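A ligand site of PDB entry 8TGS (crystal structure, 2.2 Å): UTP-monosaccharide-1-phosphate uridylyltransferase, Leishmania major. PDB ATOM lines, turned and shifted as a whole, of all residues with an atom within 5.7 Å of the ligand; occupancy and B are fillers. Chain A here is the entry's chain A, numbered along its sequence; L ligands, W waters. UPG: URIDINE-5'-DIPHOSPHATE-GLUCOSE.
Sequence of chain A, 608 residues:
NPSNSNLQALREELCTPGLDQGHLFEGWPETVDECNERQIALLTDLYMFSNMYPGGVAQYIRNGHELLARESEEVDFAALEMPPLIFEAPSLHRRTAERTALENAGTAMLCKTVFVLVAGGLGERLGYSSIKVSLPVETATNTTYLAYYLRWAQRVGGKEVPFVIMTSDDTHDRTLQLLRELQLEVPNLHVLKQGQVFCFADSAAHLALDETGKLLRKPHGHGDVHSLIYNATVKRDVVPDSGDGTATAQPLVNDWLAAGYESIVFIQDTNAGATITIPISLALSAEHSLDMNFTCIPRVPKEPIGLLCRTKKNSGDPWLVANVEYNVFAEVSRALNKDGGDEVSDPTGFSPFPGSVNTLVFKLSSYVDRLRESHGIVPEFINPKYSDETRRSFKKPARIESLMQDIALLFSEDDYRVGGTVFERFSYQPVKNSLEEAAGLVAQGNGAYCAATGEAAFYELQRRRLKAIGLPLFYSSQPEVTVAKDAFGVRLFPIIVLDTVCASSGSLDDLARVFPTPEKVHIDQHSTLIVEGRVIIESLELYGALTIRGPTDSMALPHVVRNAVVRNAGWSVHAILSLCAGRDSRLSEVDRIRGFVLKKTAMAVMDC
The side-chain carboxylate (OE2) of Glu 325 sits at hydrogen-bond distance from an oxygen (O3') of the ligand.
O3C of the ligand lies within hydrogen-bond range of N of Asp 269.
N of Gly 120 sits at hydrogen-bond distance from O2 of the ligand.
An oxygen (O4) of the ligand lies close to the backbone NH (N) of Gly 221 (3.4 Å).
An oxygen (O2A) of the ligand is in salt-bridge range of the side-chain amino group of Lys 432 (2.7 Å).
NE2 of His 222 lies within hydrogen-bond range of O1B of the ligand.
The side-chain carboxylate (OD2) of Asp 269 sits at hydrogen-bond distance from an oxygen (O2C) of the ligand (2.9 Å).
The backbone carbonyl oxygen of Ser 356 lies within hydrogen-bond range of an oxygen (O4') of the ligand, 2.7 Å away.
The side-chain amide oxygen (OE1) of Gln 268 lies close to an oxygen (O5') of the ligand, 2.9 Å away.
An oxygen (O2C) of the ligand sits at hydrogen-bond distance from the backbone NH (N) of Gly 121, 3.0 Å away.
The side-chain amide nitrogen of Gln 405 sits at hydrogen-bond distance from an oxygen (O2') of the ligand (3.0 Å).
O of Val 118 sits at hydrogen-bond distance from O3C of the ligand (2.6 Å).
A nitrogen (N3) of the ligand lies within hydrogen-bond range of the side-chain amide oxygen (OE1) of Gln 194, at 3.0 Å.
OH of Tyr 428 sits at hydrogen-bond distance from O6' of the ligand, 2.8 Å away.
An oxygen (O2) of the ligand sits at hydrogen-bond distance from the backbone NH (N) of Ala 119.
The backbone NH of Gly 306 lies within hydrogen-bond range of an oxygen (O4') of the ligand (3.1 Å).
Water W2 bridges the side-chain amide oxygen of Gln 268 and an oxygen (O6') of the ligand.
The backbone carbonyl oxygen (O) of Met 166 is in hydrogen-bond range of the backbone NH (N) of Gly 120 (3.4 Å).
The side-chain amide oxygen (OE1) of Gln 405 sits at hydrogen-bond distance from the side-chain amide nitrogen (ND2) of Asn 358 (3.2 Å).
The backbone carbonyl oxygen (O) of Gly 221 lies within hydrogen-bond range of the side-chain amide nitrogen (NE2) of Gln 194.
The backbone carbonyl oxygen of Gly 306 sits at hydrogen-bond distance from the backbone NH of Ser 356 (2.9 Å).
N of Ala 119 is in hydrogen-bond range of O of Met 166 (2.8 Å).
O of Leu 117 sits at hydrogen-bond distance from N of Met 166.
The backbone carbonyl oxygen (O) of Ile 267 lies within hydrogen-bond range of the backbone NH (N) of Val 118, 3.1 Å away.
NZ of Lys 132 is in salt-bridge range of OD1 of Asp 269.
Met 166 touches the ligand (CE to O2, 3.5 Å).
Pro 219 touches the ligand.
Ile 305 touches the ligand (CA to O4', 3.3 Å).
Asn 323 touches the ligand (ND2 to O3', 3.8 Å).
OH of Tyr 326 touches O2B of the ligand, at 3.6 Å.
O of Val 357 touches C6' of the ligand, 3.6 Å away.
Asn 358 touches the ligand.
Hydrophobic or aromatic side chains that line the ligand: Val 118, Met 166, Pro 219, His 222, Ile 305 and Tyr 428.
Of the 31 residues printed, 22 come within 4 Å of the ligand.
The nearest printed residue that does not touch the ligand is Leu 403 (4.2 Å).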
ATOM      1  N   LEU A 117      13.976  10.927  -3.939  1.00  0.00           N
ATOM      2  CA  LEU A 117      15.375  10.472  -3.965  1.00  0.00           C
ATOM      3  C   LEU A 117      15.396   8.951  -3.920  1.00  0.00           C
ATOM      4  O   LEU A 117      14.843   8.370  -2.967  1.00  0.00           O
ATOM      5  CB  LEU A 117      16.142  11.060  -2.784  1.00  0.00           C
ATOM      6  CG  LEU A 117      17.481  10.378  -2.455  1.00  0.00           C
ATOM      7  CD1 LEU A 117      18.487  10.526  -3.594  1.00  0.00           C
ATOM      8  CD2 LEU A 117      18.071  10.984  -1.218  1.00  0.00           C
ATOM      9  N   VAL A 118      16.029   8.347  -4.914  1.00  0.00           N
ATOM     10  CA  VAL A 118      16.181   6.870  -4.969  1.00  0.00           C
ATOM     11  C   VAL A 118      17.510   6.531  -4.317  1.00  0.00           C
ATOM     12  O   VAL A 118      18.544   6.995  -4.816  1.00  0.00           O
ATOM     13  CB  VAL A 118      16.076   6.344  -6.413  1.00  0.00           C
ATOM     14  CG1 VAL A 118      14.651   6.483  -6.918  1.00  0.00           C
ATOM     15  CG2 VAL A 118      17.011   7.056  -7.391  1.00  0.00           C
ATOM     16  N   ALA A 119      17.457   5.782  -3.225  1.00  0.00           N
ATOM     17  CA  ALA A 119      18.640   5.472  -2.404  1.00  0.00           C
ATOM     18  C   ALA A 119      18.559   4.038  -1.907  1.00  0.00           C
ATOM     19  O   ALA A 119      18.862   3.827  -0.703  1.00  0.00           O
ATOM     20  CB  ALA A 119      18.750   6.450  -1.282  1.00  0.00           C
ATOM     21  N   GLY A 120      18.228   3.101  -2.787  1.00  0.00           N
ATOM     22  CA  GLY A 120      18.200   1.671  -2.427  1.00  0.00           C
ATOM     23  C   GLY A 120      19.480   0.942  -2.810  1.00  0.00           C
ATOM     24  O   GLY A 120      19.683  -0.175  -2.331  1.00  0.00           O
ATOM     25  N   GLY A 121      20.334   1.547  -3.634  1.00  0.00           N
ATOM     26  CA  GLY A 121      21.521   0.886  -4.206  1.00  0.00           C
ATOM     27  C   GLY A 121      22.674   0.853  -3.237  1.00  0.00           C
ATOM     28  O   GLY A 121      22.801   1.774  -2.409  1.00  0.00           O
ATOM     29  N   LEU A 122      23.532  -0.161  -3.369  1.00  0.00           N
ATOM     30  CA  LEU A 122      24.728  -0.348  -2.499  1.00  0.00           C
ATOM     31  C   LEU A 122      25.947   0.401  -3.044  1.00  0.00           C
ATOM     32  O   LEU A 122      26.544   1.211  -2.281  1.00  0.00           O
ATOM     33  CB  LEU A 122      25.045  -1.841  -2.410  1.00  0.00           C
ATOM     34  CG  LEU A 122      23.977  -2.702  -1.751  1.00  0.00           C
ATOM     35  CD1 LEU A 122      24.073  -4.148  -2.215  1.00  0.00           C
ATOM     36  CD2 LEU A 122      24.181  -2.610  -0.259  1.00  0.00           C
ATOM     37  N   LYS A 132      25.452   5.083   0.469  1.00  0.00           N
ATOM     38  CA  LYS A 132      26.069   6.128  -0.365  1.00  0.00           C
ATOM     39  C   LYS A 132      25.609   7.535   0.033  1.00  0.00           C
ATOM     40  O   LYS A 132      26.391   8.451  -0.203  1.00  0.00           O
ATOM     41  CB  LYS A 132      25.796   5.832  -1.830  1.00  0.00           C
ATOM     42  CG  LYS A 132      26.531   4.582  -2.308  1.00  0.00           C
ATOM     43  CD  LYS A 132      26.335   4.299  -3.754  1.00  0.00           C
ATOM     44  CE  LYS A 132      26.959   5.348  -4.632  1.00  0.00           C
ATOM     45  NZ  LYS A 132      26.755   5.018  -6.066  1.00  0.00           N
ATOM     46  N   MET A 166      13.318   6.504  -1.379  1.00  0.00           N
ATOM     47  CA  MET A 166      13.224   5.043  -1.572  1.00  0.00           C
ATOM     48  C   MET A 166      14.477   4.389  -1.019  1.00  0.00           C
ATOM     49  O   MET A 166      15.617   4.758  -1.405  1.00  0.00           O
ATOM     50  CB  MET A 166      13.042   4.662  -3.038  1.00  0.00           C
ATOM     51  CG  MET A 166      12.719   3.184  -3.187  1.00  0.00           C
ATOM     52  SD  MET A 166      12.323   2.653  -4.856  1.00  0.00           S
ATOM     53  CE  MET A 166      13.945   2.708  -5.605  1.00  0.00           C
ATOM     54  N   GLN A 194      11.649  -0.555  -0.882  1.00  0.00           N
ATOM     55  CA  GLN A 194      11.390  -1.502  -1.986  1.00  0.00           C
ATOM     56  C   GLN A 194      11.695  -2.914  -1.500  1.00  0.00           C
ATOM     57  O   GLN A 194      12.555  -3.091  -0.607  1.00  0.00           O
ATOM     58  CB  GLN A 194      12.194  -1.161  -3.244  1.00  0.00           C
ATOM     59  CG  GLN A 194      13.676  -1.449  -3.136  1.00  0.00           C
ATOM     60  CD  GLN A 194      14.463  -0.848  -4.287  1.00  0.00           C
ATOM     61  OE1 GLN A 194      15.427  -0.118  -4.080  1.00  0.00           O
ATOM     62  NE2 GLN A 194      14.048  -1.134  -5.514  1.00  0.00           N
ATOM     63  N   PRO A 219      17.909  -7.181  -6.045  1.00  0.00           N
ATOM     64  CA  PRO A 219      17.160  -5.950  -6.322  1.00  0.00           C
ATOM     65  C   PRO A 219      16.379  -5.861  -7.638  1.00  0.00           C
ATOM     66  O   PRO A 219      16.854  -6.348  -8.622  1.00  0.00           O
ATOM     67  CB  PRO A 219      18.276  -4.884  -6.310  1.00  0.00           C
ATOM     68  CG  PRO A 219      19.416  -5.524  -5.560  1.00  0.00           C
ATOM     69  CD  PRO A 219      19.358  -6.961  -6.000  1.00  0.00           C
ATOM     70  N   HIS A 220      15.229  -5.194  -7.601  1.00  0.00           N
ATOM     71  CA  HIS A 220      14.353  -5.059  -8.784  1.00  0.00           C
ATOM     72  C   HIS A 220      14.621  -3.720  -9.494  1.00  0.00           C
ATOM     73  O   HIS A 220      13.852  -3.401 -10.415  1.00  0.00           O
ATOM     74  CB  HIS A 220      12.889  -5.179  -8.360  1.00  0.00           C
ATOM     75  CG  HIS A 220      11.938  -5.297  -9.495  1.00  0.00           C
ATOM     76  ND1 HIS A 220      11.115  -4.258  -9.894  1.00  0.00           N
ATOM     77  CD2 HIS A 220      11.678  -6.322 -10.335  1.00  0.00           C
ATOM     78  CE1 HIS A 220      10.386  -4.645 -10.926  1.00  0.00           C
ATOM     79  NE2 HIS A 220      10.715  -5.911 -11.208  1.00  0.00           N
ATOM     80  N   GLY A 221      15.623  -2.965  -9.075  1.00  0.00           N
ATOM     81  CA  GLY A 221      15.991  -1.709  -9.754  1.00  0.00           C
ATOM     82  C   GLY A 221      15.186  -0.531  -9.237  1.00  0.00           C
ATOM     83  O   GLY A 221      14.234  -0.711  -8.465  1.00  0.00           O
ATOM     84  N   HIS A 222      15.564   0.649  -9.688  1.00  0.00           N
ATOM     85  CA  HIS A 222      14.974   1.906  -9.185  1.00  0.00           C
ATOM     86  C   HIS A 222      13.597   2.123  -9.796  1.00  0.00           C
ATOM     87  O   HIS A 222      12.996   3.132  -9.451  1.00  0.00           O
ATOM     88  CB  HIS A 222      15.880   3.117  -9.454  1.00  0.00           C
ATOM     89  CG  HIS A 222      16.617   3.085 -10.752  1.00  0.00           C
ATOM     90  ND1 HIS A 222      16.018   3.340 -11.959  1.00  0.00           N
ATOM     91  CD2 HIS A 222      17.912   2.830 -11.028  1.00  0.00           C
ATOM     92  CE1 HIS A 222      16.901   3.254 -12.918  1.00  0.00           C
ATOM     93  NE2 HIS A 222      18.086   2.933 -12.375  1.00  0.00           N
ATOM     94  N   ILE A 267      15.692  12.297  -8.171  1.00  0.00           N
ATOM     95  CA  ILE A 267      17.167  12.455  -8.152  1.00  0.00           C
ATOM     96  C   ILE A 267      17.787  11.144  -7.686  1.00  0.00           C
ATOM     97  O   ILE A 267      17.115  10.368  -7.037  1.00  0.00           O
ATOM     98  CB  ILE A 267      17.594  13.611  -7.239  1.00  0.00           C
ATOM     99  CG1 ILE A 267      16.991  13.456  -5.830  1.00  0.00           C
ATOM    100  CG2 ILE A 267      17.191  14.937  -7.855  1.00  0.00           C
ATOM    101  CD1 ILE A 267      17.705  14.295  -4.806  1.00  0.00           C
ATOM    102  N   GLN A 268      19.084  11.018  -7.940  1.00  0.00           N
ATOM    103  CA  GLN A 268      19.895   9.856  -7.558  1.00  0.00           C
ATOM    104  C   GLN A 268      20.790  10.235  -6.369  1.00  0.00           C
ATOM    105  O   GLN A 268      20.809  11.428  -5.967  1.00  0.00           O
ATOM    106  CB  GLN A 268      20.710   9.362  -8.753  1.00  0.00           C
ATOM    107  CG  GLN A 268      19.852   9.096  -9.992  1.00  0.00           C
ATOM    108  CD  GLN A 268      20.396   8.055 -10.958  1.00  0.00           C
ATOM    109  OE1 GLN A 268      21.573   8.054 -11.356  1.00  0.00           O
ATOM    110  NE2 GLN A 268      19.555   7.111 -11.320  1.00  0.00           N
ATOM    111  N   ASP A 269      21.501   9.253  -5.850  1.00  0.00           N
ATOM    112  CA  ASP A 269      22.039   9.300  -4.477  1.00  0.00           C
ATOM    113  C   ASP A 269      23.319  10.130  -4.389  1.00  0.00           C
ATOM    114  O   ASP A 269      23.520  10.671  -3.282  1.00  0.00           O
ATOM    115  CB  ASP A 269      22.346   7.895  -3.946  1.00  0.00           C
ATOM    116  CG  ASP A 269      23.024   6.959  -4.933  1.00  0.00           C
ATOM    117  OD1 ASP A 269      23.614   7.424  -5.908  1.00  0.00           O
ATOM    118  OD2 ASP A 269      22.922   5.759  -4.706  1.00  0.00           O
ATOM    119  N   THR A 270      24.142  10.246  -5.450  1.00  0.00           N
ATOM    120  CA  THR A 270      25.446  10.918  -5.280  1.00  0.00           C
ATOM    121  C   THR A 270      25.759  11.932  -6.363  1.00  0.00           C
ATOM    122  O   THR A 270      26.950  12.034  -6.716  1.00  0.00           O
ATOM    123  CB  THR A 270      26.593   9.911  -5.196  1.00  0.00           C
ATOM    124  OG1 THR A 270      26.769   9.204  -6.426  1.00  0.00           O
ATOM    125  CG2 THR A 270      26.388   8.949  -4.040  1.00  0.00           C
ATOM    126  N   PRO A 304      29.136   5.132 -19.505  1.00  0.00           N
ATOM    127  CA  PRO A 304      28.064   4.336 -18.926  1.00  0.00           C
ATOM    128  C   PRO A 304      26.863   5.192 -18.484  1.00  0.00           C
ATOM    129  O   PRO A 304      26.422   5.082 -17.351  1.00  0.00           O
ATOM    130  CB  PRO A 304      28.715   3.621 -17.737  1.00  0.00           C
ATOM    131  CG  PRO A 304      30.197   3.948 -17.830  1.00  0.00           C
ATOM    132  CD  PRO A 304      30.296   5.235 -18.602  1.00  0.00           C
ATOM    133  N   ILE A 305      26.339   5.999 -19.410  1.00  0.00           N
ATOM    134  CA  ILE A 305      25.065   6.732 -19.215  1.00  0.00           C
ATOM    135  C   ILE A 305      24.151   6.445 -20.406  1.00  0.00           C
ATOM    136  O   ILE A 305      24.666   6.244 -21.527  1.00  0.00           O
ATOM    137  CB  ILE A 305      25.292   8.245 -19.044  1.00  0.00           C
ATOM    138  CG1 ILE A 305      25.818   8.872 -20.336  1.00  0.00           C
ATOM    139  CG2 ILE A 305      26.225   8.509 -17.876  1.00  0.00           C
ATOM    140  CD1 ILE A 305      25.998  10.358 -20.265  1.00  0.00           C
ATOM    141  N   GLY A 306      22.847   6.470 -20.165  1.00  0.00           N
ATOM    142  CA  GLY A 306      21.859   6.230 -21.220  1.00  0.00           C
ATOM    143  C   GLY A 306      21.810   7.363 -22.230  1.00  0.00           C
ATOM    144  O   GLY A 306      22.429   8.428 -21.999  1.00  0.00           O
ATOM    145  N   ASN A 323      14.556   6.661 -22.957  1.00  0.00           N
ATOM    146  CA  ASN A 323      15.997   6.474 -22.709  1.00  0.00           C
ATOM    147  C   ASN A 323      16.388   5.118 -23.267  1.00  0.00           C
ATOM    148  O   ASN A 323      15.625   4.144 -23.041  1.00  0.00           O
ATOM    149  CB  ASN A 323      16.319   6.567 -21.215  1.00  0.00           C
ATOM    150  CG  ASN A 323      17.733   6.154 -20.919  1.00  0.00           C
ATOM    151  OD1 ASN A 323      18.680   6.887 -21.186  1.00  0.00           O
ATOM    152  ND2 ASN A 323      17.889   4.958 -20.367  1.00  0.00           N
ATOM    153  N   GLU A 325      19.494   2.591 -22.745  1.00  0.00           N
ATOM    154  CA  GLU A 325      20.645   2.367 -21.836  1.00  0.00           C
ATOM    155  C   GLU A 325      21.913   2.155 -22.659  1.00  0.00           C
ATOM    156  O   GLU A 325      21.838   1.828 -23.843  1.00  0.00           O
ATOM    157  CB  GLU A 325      20.383   1.182 -20.903  1.00  0.00           C
ATOM    158  CG  GLU A 325      19.631   1.568 -19.639  1.00  0.00           C
ATOM    159  CD  GLU A 325      20.243   2.693 -18.800  1.00  0.00           C
ATOM    160  OE1 GLU A 325      20.714   2.401 -17.688  1.00  0.00           O
ATOM    161  OE2 GLU A 325      20.190   3.866 -19.240  1.00  0.00           O
ATOM    162  N   TYR A 326      23.069   2.374 -22.041  1.00  0.00           N
ATOM    163  CA  TYR A 326      24.364   2.328 -22.776  1.00  0.00           C
ATOM    164  C   TYR A 326      24.579   0.960 -23.426  1.00  0.00           C
ATOM    165  O   TYR A 326      25.067   0.921 -24.572  1.00  0.00           O
ATOM    166  CB  TYR A 326      25.508   2.645 -21.822  1.00  0.00           C
ATOM    167  CG  TYR A 326      25.336   2.144 -20.405  1.00  0.00           C
ATOM    168  CD1 TYR A 326      24.463   2.759 -19.530  1.00  0.00           C
ATOM    169  CD2 TYR A 326      26.050   1.046 -19.950  1.00  0.00           C
ATOM    170  CE1 TYR A 326      24.311   2.305 -18.228  1.00  0.00           C
ATOM    171  CE2 TYR A 326      25.897   0.574 -18.663  1.00  0.00           C
ATOM    172  CZ  TYR A 326      25.028   1.212 -17.794  1.00  0.00           C
ATOM    173  OH  TYR A 326      24.874   0.741 -16.507  1.00  0.00           O
ATOM    174  N   SER A 356      21.547  10.924 -20.862  1.00  0.00           N
ATOM    175  CA  SER A 356      20.575  11.181 -19.772  1.00  0.00           C
ATOM    176  C   SER A 356      21.234  10.910 -18.416  1.00  0.00           C
ATOM    177  O   SER A 356      21.732   9.785 -18.196  1.00  0.00           O
ATOM    178  CB  SER A 356      19.360  10.347 -19.928  1.00  0.00           C
ATOM    179  OG  SER A 356      18.468  10.546 -18.859  1.00  0.00           O
ATOM    180  N   VAL A 357      21.235  11.906 -17.534  1.00  0.00           N
ATOM    181  CA  VAL A 357      21.854  11.778 -16.181  1.00  0.00           C
ATOM    182  C   VAL A 357      20.808  11.316 -15.164  1.00  0.00           C
ATOM    183  O   VAL A 357      21.169  11.097 -14.016  1.00  0.00           O
ATOM    184  CB  VAL A 357      22.505  13.102 -15.752  1.00  0.00           C
ATOM    185  CG1 VAL A 357      23.481  13.598 -16.801  1.00  0.00           C
ATOM    186  CG2 VAL A 357      21.472  14.175 -15.455  1.00  0.00           C
ATOM    187  N   ASN A 358      19.562  11.129 -15.567  1.00  0.00           N
ATOM    188  CA  ASN A 358      18.492  10.552 -14.702  1.00  0.00           C
ATOM    189  C   ASN A 358      18.185  11.531 -13.552  1.00  0.00           C
ATOM    190  O   ASN A 358      18.001  11.135 -12.387  1.00  0.00           O
ATOM    191  CB  ASN A 358      18.858   9.165 -14.177  1.00  0.00           C
ATOM    192  CG  ASN A 358      17.808   8.103 -14.494  1.00  0.00           C
ATOM    193  OD1 ASN A 358      17.018   8.244 -15.422  1.00  0.00           O
ATOM    194  ND2 ASN A 358      17.830   7.007 -13.760  1.00  0.00           N
ATOM    195  N   LEU A 403      13.593   0.145 -14.615  1.00  0.00           N
ATOM    196  CA  LEU A 403      14.224   1.491 -14.620  1.00  0.00           C
ATOM    197  C   LEU A 403      13.136   2.526 -14.390  1.00  0.00           C
ATOM    198  O   LEU A 403      12.057   2.425 -15.027  1.00  0.00           O
ATOM    199  CB  LEU A 403      14.910   1.787 -15.946  1.00  0.00           C
ATOM    200  CG  LEU A 403      15.970   0.790 -16.418  1.00  0.00           C
ATOM    201  CD1 LEU A 403      16.448   1.205 -17.792  1.00  0.00           C
ATOM    202  CD2 LEU A 403      17.145   0.723 -15.466  1.00  0.00           C
ATOM    203  N   GLN A 405      13.222   5.662 -15.180  1.00  0.00           N
ATOM    204  CA  GLN A 405      13.077   6.540 -16.353  1.00  0.00           C
ATOM    205  C   GLN A 405      12.241   5.853 -17.436  1.00  0.00           C
ATOM    206  O   GLN A 405      11.753   6.572 -18.333  1.00  0.00           O
ATOM    207  CB  GLN A 405      14.435   6.975 -16.887  1.00  0.00           C
ATOM    208  CG  GLN A 405      15.283   5.861 -17.500  1.00  0.00           C
ATOM    209  CD  GLN A 405      16.210   5.240 -16.495  1.00  0.00           C
ATOM    210  OE1 GLN A 405      15.858   5.039 -15.340  1.00  0.00           O
ATOM    211  NE2 GLN A 405      17.405   4.899 -16.943  1.00  0.00           N
ATOM    212  N   TYR A 428      27.268  17.412 -14.098  1.00  0.00           N
ATOM    213  CA  TYR A 428      27.018  15.988 -13.767  1.00  0.00           C
ATOM    214  C   TYR A 428      28.207  15.515 -12.958  1.00  0.00           C
ATOM    215  O   TYR A 428      29.308  15.374 -13.550  1.00  0.00           O
ATOM    216  CB  TYR A 428      26.788  15.176 -15.033  1.00  0.00           C
ATOM    217  CG  TYR A 428      26.634  13.681 -14.852  1.00  0.00           C
ATOM    218  CD1 TYR A 428      25.625  13.173 -14.057  1.00  0.00           C
ATOM    219  CD2 TYR A 428      27.500  12.791 -15.436  1.00  0.00           C
ATOM    220  CE1 TYR A 428      25.464  11.806 -13.885  1.00  0.00           C
ATOM    221  CE2 TYR A 428      27.359  11.418 -15.273  1.00  0.00           C
ATOM    222  CZ  TYR A 428      26.330  10.925 -14.499  1.00  0.00           C
ATOM    223  OH  TYR A 428      26.250   9.577 -14.329  1.00  0.00           O
ATOM    224  N   PRO A 430      28.619  12.632 -10.411  1.00  0.00           N
ATOM    225  CA  PRO A 430      28.341  11.478  -9.585  1.00  0.00           C
ATOM    226  C   PRO A 430      29.611  10.891  -8.966  1.00  0.00           C
ATOM    227  O   PRO A 430      30.735  11.095  -9.509  1.00  0.00           O
ATOM    228  CB  PRO A 430      27.714  10.495 -10.590  1.00  0.00           C
ATOM    229  CG  PRO A 430      28.441  10.814 -11.870  1.00  0.00           C
ATOM    230  CD  PRO A 430      28.643  12.319 -11.856  1.00  0.00           C
ATOM    231  N   LYS A 432      30.647   7.292  -8.488  1.00  0.00           N
ATOM    232  CA  LYS A 432      30.284   5.914  -8.914  1.00  0.00           C
ATOM    233  C   LYS A 432      31.486   4.962  -8.857  1.00  0.00           C
ATOM    234  O   LYS A 432      31.267   3.797  -8.503  1.00  0.00           O
ATOM    235  CB  LYS A 432      29.765   5.950 -10.348  1.00  0.00           C
ATOM    236  CG  LYS A 432      28.455   6.690 -10.509  1.00  0.00           C
ATOM    237  CD  LYS A 432      27.445   5.931 -11.341  1.00  0.00           C
ATOM    238  CE  LYS A 432      26.103   6.626 -11.394  1.00  0.00           C
ATOM    239  NZ  LYS A 432      25.041   5.755 -11.974  1.00  0.00           N
HETATM  240  N1  UPG L   1      18.738   2.496  -7.071  1.00  0.00           N
HETATM  241  C2  UPG L   1      17.834   2.210  -6.069  1.00  0.00           C
HETATM  242  N3  UPG L   1      17.429   0.900  -6.036  1.00  0.00           N
HETATM  243  C4  UPG L   1      17.829  -0.121  -6.870  1.00  0.00           C
HETATM  244  C5  UPG L   1      18.768   0.262  -7.869  1.00  0.00           C
HETATM  245  C6  UPG L   1      19.182   1.531  -7.938  1.00  0.00           C
HETATM  246  O2  UPG L   1      17.418   3.049  -5.298  1.00  0.00           O
HETATM  247  O4  UPG L   1      17.374  -1.244  -6.705  1.00  0.00           O
HETATM  248  C1C UPG L   1      19.214   3.886  -7.173  1.00  0.00           C
HETATM  249  C2C UPG L   1      20.601   4.092  -6.608  1.00  0.00           C
HETATM  250  O2C UPG L   1      20.597   4.144  -5.195  1.00  0.00           O
HETATM  251  C3C UPG L   1      20.938   5.433  -7.265  1.00  0.00           C
HETATM  252  C4C UPG L   1      20.306   5.279  -8.664  1.00  0.00           C
HETATM  253  O4C UPG L   1      19.352   4.200  -8.540  1.00  0.00           O
HETATM  254  O3C UPG L   1      20.350   6.504  -6.559  1.00  0.00           O
HETATM  255  C5C UPG L   1      21.235   4.983  -9.815  1.00  0.00           C
HETATM  256  O5C UPG L   1      21.813   3.676  -9.661  1.00  0.00           O
HETATM  257  PA  UPG L   1      23.270   3.510 -10.288  1.00  0.00           P
HETATM  258  O1A UPG L   1      23.694   2.087 -10.186  1.00  0.00           O
HETATM  259  O2A UPG L   1      24.169   4.544  -9.716  1.00  0.00           O
HETATM  260  O3A UPG L   1      23.010   3.864 -11.819  1.00  0.00           O
HETATM  261  PB  UPG L   1      22.399   3.044 -13.050  1.00  0.00           P
HETATM  262  O1B UPG L   1      21.056   2.519 -12.665  1.00  0.00           O
HETATM  263  O2B UPG L   1      23.419   2.059 -13.505  1.00  0.00           O
HETATM  264  O3B UPG L   1      22.203   4.172 -14.162  1.00  0.00           O
HETATM  265  C1' UPG L   1      21.277   5.210 -13.956  1.00  0.00           C
HETATM  266  C2' UPG L   1      20.355   5.264 -15.166  1.00  0.00           C
HETATM  267  C3' UPG L   1      21.117   5.706 -16.393  1.00  0.00           C
HETATM  268  C4' UPG L   1      21.796   7.026 -16.117  1.00  0.00           C
HETATM  269  C5' UPG L   1      22.700   6.898 -14.909  1.00  0.00           C
HETATM  270  C6' UPG L   1      23.320   8.217 -14.514  1.00  0.00           C
HETATM  271  O2' UPG L   1      19.739   4.003 -15.373  1.00  0.00           O
HETATM  272  O3' UPG L   1      20.213   5.844 -17.489  1.00  0.00           O
HETATM  273  O4' UPG L   1      22.569   7.409 -17.243  1.00  0.00           O
HETATM  274  O5' UPG L   1      21.930   6.451 -13.779  1.00  0.00           O
HETATM  275  O6' UPG L   1      24.114   8.092 -13.354  1.00  0.00           O
HETATM  276  O   HOH W   1      21.824   4.382  -2.072  1.00  0.00           O
HETATM  277  O   HOH W   2      23.769   9.957 -10.998  1.00  0.00           O
